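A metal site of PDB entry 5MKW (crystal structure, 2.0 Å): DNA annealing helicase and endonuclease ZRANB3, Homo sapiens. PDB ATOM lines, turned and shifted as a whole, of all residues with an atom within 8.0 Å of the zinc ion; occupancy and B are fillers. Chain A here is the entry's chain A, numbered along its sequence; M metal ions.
The backbone NH of Val 25 lies close to the side-chain sulfur of Cys 23 (3.8 Å).
O of Val 25 is in hydrogen-bond range of N of Cys 20, 2.9 Å away.
The backbone NH (N) of Leu 22 lies close to the side-chain sulfur (SG) of Cys 20, 3.5 Å away.
The backbone carbonyl oxygen (O) of Cys 20 sits close to the side-chain amide oxygen (OD1) of Asn 24 (2.9 Å).
N of Val 98 lies close to SG of Cys 96, 3.7 Å away.
Of the 19 residues printed, 4 come within 4 Å of the zinc ion.
The zinc ion is bound by the side-chain sulfur (SG) of Cys 99 (2.3 Å), the side-chain sulfur (SG) of Cys 23 (2.3 Å), the side-chain sulfur (SG) of Cys 20 (2.4 Å) and the side-chain sulfur (SG) of Cys 96 (2.4 Å).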
ATOM      1  N   VAL A  19      26.727  24.729  24.792  1.00  0.00           N
ATOM      2  CA  VAL A  19      25.538  23.900  25.112  1.00  0.00           C
ATOM      3  C   VAL A  19      24.871  23.382  23.853  1.00  0.00           C
ATOM      4  O   VAL A  19      24.637  24.157  22.897  1.00  0.00           O
ATOM      5  CB  VAL A  19      24.484  24.703  25.880  1.00  0.00           C
ATOM      6  CG1 VAL A  19      23.278  23.819  26.206  1.00  0.00           C
ATOM      7  CG2 VAL A  19      25.104  25.245  27.164  1.00  0.00           C
ATOM      8  N   CYS A  20      24.760  22.074  23.734  1.00  0.00           N
ATOM      9  CA  CYS A  20      24.258  21.471  22.491  1.00  0.00           C
ATOM     10  C   CYS A  20      22.799  21.874  22.290  1.00  0.00           C
ATOM     11  O   CYS A  20      21.981  21.766  23.242  1.00  0.00           O
ATOM     12  CB  CYS A  20      24.303  19.949  22.539  1.00  0.00           C
ATOM     13  SG  CYS A  20      23.694  19.136  21.043  1.00  0.00           S
ATOM     14  N   GLN A  21      22.481  22.349  21.093  1.00  0.00           N
ATOM     15  CA  GLN A  21      21.140  22.879  20.842  1.00  0.00           C
ATOM     16  C   GLN A  21      20.144  21.793  20.508  1.00  0.00           C
ATOM     17  O   GLN A  21      18.947  22.058  20.504  1.00  0.00           O
ATOM     18  CB  GLN A  21      21.194  23.920  19.733  1.00  0.00           C
ATOM     19  CG  GLN A  21      22.034  25.114  20.100  1.00  0.00           C
ATOM     20  CD  GLN A  21      21.523  25.811  21.393  1.00  0.00           C
ATOM     21  OE1 GLN A  21      20.458  26.416  21.391  1.00  0.00           O
ATOM     22  NE2 GLN A  21      22.283  25.718  22.467  1.00  0.00           N
ATOM     23  N   LEU A  22      20.616  20.559  20.310  1.00  0.00           N
ATOM     24  CA  LEU A  22      19.726  19.407  20.088  1.00  0.00           C
ATOM     25  C   LEU A  22      19.402  18.643  21.359  1.00  0.00           C
ATOM     26  O   LEU A  22      18.247  18.313  21.574  1.00  0.00           O
ATOM     27  CB  LEU A  22      20.272  18.461  19.031  1.00  0.00           C
ATOM     28  CG  LEU A  22      20.516  19.125  17.673  1.00  0.00           C
ATOM     29  CD1 LEU A  22      20.916  18.136  16.604  1.00  0.00           C
ATOM     30  CD2 LEU A  22      19.304  19.949  17.243  1.00  0.00           C
ATOM     31  N   CYS A  23      20.419  18.329  22.166  1.00  0.00           N
ATOM     32  CA  CYS A  23      20.224  17.474  23.325  1.00  0.00           C
ATOM     33  C   CYS A  23      20.483  18.173  24.663  1.00  0.00           C
ATOM     34  O   CYS A  23      20.196  17.604  25.695  1.00  0.00           O
ATOM     35  CB  CYS A  23      21.114  16.224  23.214  1.00  0.00           C
ATOM     36  SG  CYS A  23      22.846  16.534  23.580  1.00  0.00           S
ATOM     37  N   ASN A  24      20.993  19.393  24.605  1.00  0.00           N
ATOM     38  CA  ASN A  24      21.164  20.311  25.727  1.00  0.00           C
ATOM     39  C   ASN A  24      22.184  19.879  26.772  1.00  0.00           C
ATOM     40  O   ASN A  24      22.275  20.471  27.839  1.00  0.00           O
ATOM     41  CB  ASN A  24      19.821  20.771  26.292  1.00  0.00           C
ATOM     42  CG  ASN A  24      18.953  21.415  25.216  1.00  0.00           C
ATOM     43  OD1 ASN A  24      19.389  22.351  24.495  1.00  0.00           O
ATOM     44  ND2 ASN A  24      17.803  20.806  24.966  1.00  0.00           N
ATOM     45  N   VAL A  25      23.094  19.017  26.386  1.00  0.00           N
ATOM     46  CA  VAL A  25      24.229  18.797  27.242  1.00  0.00           C
ATOM     47  C   VAL A  25      25.129  20.012  27.273  1.00  0.00           C
ATOM     48  O   VAL A  25      25.240  20.774  26.293  1.00  0.00           O
ATOM     49  CB  VAL A  25      25.029  17.526  26.892  1.00  0.00           C
ATOM     50  CG1 VAL A  25      24.138  16.299  27.031  1.00  0.00           C
ATOM     51  CG2 VAL A  25      25.692  17.626  25.522  1.00  0.00           C
ATOM     52  N   ASN A  26      25.750  20.232  28.426  1.00  0.00           N
ATOM     53  CA  ASN A  26      26.716  21.333  28.514  1.00  0.00           C
ATOM     54  C   ASN A  26      28.112  20.811  28.220  1.00  0.00           C
ATOM     55  O   ASN A  26      28.809  20.301  29.098  1.00  0.00           O
ATOM     56  CB  ASN A  26      26.677  22.045  29.876  1.00  0.00           C
ATOM     57  CG  ASN A  26      27.543  23.288  29.861  1.00  0.00           C
ATOM     58  OD1 ASN A  26      28.522  23.413  29.115  1.00  0.00           O
ATOM     59  ND2 ASN A  26      27.121  24.260  30.604  1.00  0.00           N
ATOM     60  N   ALA A  27      28.453  20.829  26.931  1.00  0.00           N
ATOM     61  CA  ALA A  27      29.618  20.136  26.462  1.00  0.00           C
ATOM     62  C   ALA A  27      30.870  20.858  26.909  1.00  0.00           C
ATOM     63  O   ALA A  27      31.891  20.225  27.214  1.00  0.00           O
ATOM     64  CB  ALA A  27      29.563  20.004  24.957  1.00  0.00           C
ATOM     65  N   TRP A  50      27.415  11.040  28.326  1.00  0.00           N
ATOM     66  CA  TRP A  50      27.033  11.040  26.899  1.00  0.00           C
ATOM     67  C   TRP A  50      28.196  10.837  25.961  1.00  0.00           C
ATOM     68  O   TRP A  50      28.023  10.324  24.854  1.00  0.00           O
ATOM     69  CB  TRP A  50      26.334  12.374  26.535  1.00  0.00           C
ATOM     70  CG  TRP A  50      27.202  13.614  26.767  1.00  0.00           C
ATOM     71  CD1 TRP A  50      27.197  14.438  27.853  1.00  0.00           C
ATOM     72  CD2 TRP A  50      28.101  14.204  25.843  1.00  0.00           C
ATOM     73  NE1 TRP A  50      28.065  15.490  27.676  1.00  0.00           N
ATOM     74  CE2 TRP A  50      28.650  15.352  26.447  1.00  0.00           C
ATOM     75  CE3 TRP A  50      28.454  13.933  24.533  1.00  0.00           C
ATOM     76  CZ2 TRP A  50      29.538  16.186  25.789  1.00  0.00           C
ATOM     77  CZ3 TRP A  50      29.429  14.678  23.932  1.00  0.00           C
ATOM     78  CH2 TRP A  50      29.921  15.829  24.528  1.00  0.00           C
ATOM     79  N   PHE A  71      34.509  17.918  22.241  1.00  0.00           N
ATOM     80  CA  PHE A  71      33.264  17.965  23.000  1.00  0.00           C
ATOM     81  C   PHE A  71      32.111  18.658  22.240  1.00  0.00           C
ATOM     82  O   PHE A  71      30.949  18.239  22.367  1.00  0.00           O
ATOM     83  CB  PHE A  71      33.543  18.669  24.348  1.00  0.00           C
ATOM     84  CG  PHE A  71      34.453  17.890  25.251  1.00  0.00           C
ATOM     85  CD1 PHE A  71      35.831  17.908  25.056  1.00  0.00           C
ATOM     86  CD2 PHE A  71      33.928  16.982  26.129  1.00  0.00           C
ATOM     87  CE1 PHE A  71      36.670  17.123  25.841  1.00  0.00           C
ATOM     88  CE2 PHE A  71      34.743  16.181  26.900  1.00  0.00           C
ATOM     89  CZ  PHE A  71      36.138  16.270  26.767  1.00  0.00           C
ATOM     90  N   THR A  94      25.574  25.252  18.073  1.00  0.00           N
ATOM     91  CA  THR A  94      26.424  24.363  18.806  1.00  0.00           C
ATOM     92  C   THR A  94      25.781  23.005  18.864  1.00  0.00           C
ATOM     93  O   THR A  94      24.597  22.855  19.217  1.00  0.00           O
ATOM     94  CB  THR A  94      26.598  24.910  20.254  1.00  0.00           C
ATOM     95  OG1 THR A  94      27.141  26.240  20.217  1.00  0.00           O
ATOM     96  CG2 THR A  94      27.512  24.023  21.031  1.00  0.00           C
ATOM     97  N   LEU A  95      26.587  22.013  18.523  1.00  0.00           N
ATOM     98  CA  LEU A  95      26.233  20.604  18.715  1.00  0.00           C
ATOM     99  C   LEU A  95      27.319  19.947  19.562  1.00  0.00           C
ATOM    100  O   LEU A  95      28.521  20.164  19.316  1.00  0.00           O
ATOM    101  CB  LEU A  95      26.159  19.848  17.368  1.00  0.00           C
ATOM    102  CG  LEU A  95      25.131  20.254  16.297  1.00  0.00           C
ATOM    103  CD1 LEU A  95      25.209  19.313  15.111  1.00  0.00           C
ATOM    104  CD2 LEU A  95      23.723  20.262  16.860  1.00  0.00           C
ATOM    105  N   CYS A  96      26.930  19.076  20.488  1.00  0.00           N
ATOM    106  CA  CYS A  96      27.902  18.200  21.090  1.00  0.00           C
ATOM    107  C   CYS A  96      28.439  17.255  19.988  1.00  0.00           C
ATOM    108  O   CYS A  96      27.861  17.101  18.888  1.00  0.00           O
ATOM    109  CB  CYS A  96      27.273  17.386  22.242  1.00  0.00           C
ATOM    110  SG  CYS A  96      26.164  16.073  21.730  1.00  0.00           S
ATOM    111  N   THR A  97      29.566  16.612  20.273  1.00  0.00           N
ATOM    112  CA  THR A  97      30.210  15.803  19.249  1.00  0.00           C
ATOM    113  C   THR A  97      29.448  14.518  18.916  1.00  0.00           C
ATOM    114  O   THR A  97      29.567  14.024  17.830  1.00  0.00           O
ATOM    115  CB  THR A  97      31.675  15.532  19.586  1.00  0.00           C
ATOM    116  OG1 THR A  97      31.804  15.258  20.998  1.00  0.00           O
ATOM    117  CG2 THR A  97      32.495  16.787  19.208  1.00  0.00           C
ATOM    118  N   VAL A  98      28.626  14.020  19.827  1.00  0.00           N
ATOM    119  CA  VAL A  98      27.797  12.863  19.564  1.00  0.00           C
ATOM    120  C   VAL A  98      26.666  13.241  18.586  1.00  0.00           C
ATOM    121  O   VAL A  98      26.454  12.596  17.577  1.00  0.00           O
ATOM    122  CB  VAL A  98      27.244  12.262  20.870  1.00  0.00           C
ATOM    123  CG1 VAL A  98      26.122  11.266  20.597  1.00  0.00           C
ATOM    124  CG2 VAL A  98      28.364  11.587  21.674  1.00  0.00           C
ATOM    125  N   CYS A  99      26.008  14.349  18.840  1.00  0.00           N
ATOM    126  CA  CYS A  99      25.024  14.838  17.855  1.00  0.00           C
ATOM    127  C   CYS A  99      25.661  15.211  16.499  1.00  0.00           C
ATOM    128  O   CYS A  99      25.070  15.035  15.437  1.00  0.00           O
ATOM    129  CB  CYS A  99      24.282  16.042  18.413  1.00  0.00           C
ATOM    130  SG  CYS A  99      23.168  15.636  19.798  1.00  0.00           S
ATOM    131  N   HIS A 100      26.828  15.803  16.544  1.00  0.00           N
ATOM    132  CA  HIS A 100      27.494  16.193  15.334  1.00  0.00           C
ATOM    133  C   HIS A 100      27.835  14.946  14.483  1.00  0.00           C
ATOM    134  O   HIS A 100      27.697  14.974  13.272  1.00  0.00           O
ATOM    135  CB  HIS A 100      28.745  16.953  15.636  1.00  0.00           C
ATOM    136  CG  HIS A 100      29.464  17.416  14.420  1.00  0.00           C
ATOM    137  ND1 HIS A 100      30.750  17.045  14.136  1.00  0.00           N
ATOM    138  CD2 HIS A 100      29.096  18.304  13.470  1.00  0.00           C
ATOM    139  CE1 HIS A 100      31.168  17.713  13.083  1.00  0.00           C
ATOM    140  NE2 HIS A 100      30.141  18.378  12.583  1.00  0.00           N
ATOM    141  N   GLU A 102      26.283  11.895  14.585  1.00  0.00           N
ATOM    142  CA  GLU A 102      25.010  11.402  14.031  1.00  0.00           C
ATOM    143  C   GLU A 102      24.628  12.188  12.785  1.00  0.00           C
ATOM    144  O   GLU A 102      24.197  11.622  11.783  1.00  0.00           O
ATOM    145  CB  GLU A 102      23.864  11.497  15.019  1.00  0.00           C
ATOM    146  CG  GLU A 102      23.976  10.585  16.222  1.00  0.00           C
ATOM    147  CD  GLU A 102      22.975  10.959  17.340  1.00  0.00           C
ATOM    148  OE1 GLU A 102      22.043  11.746  17.092  1.00  0.00           O
ATOM    149  OE2 GLU A 102      23.075  10.414  18.456  1.00  0.00           O
HETATM  150 ZN    ZN M   1      23.950  16.860  21.578  1.00  0.00          ZN
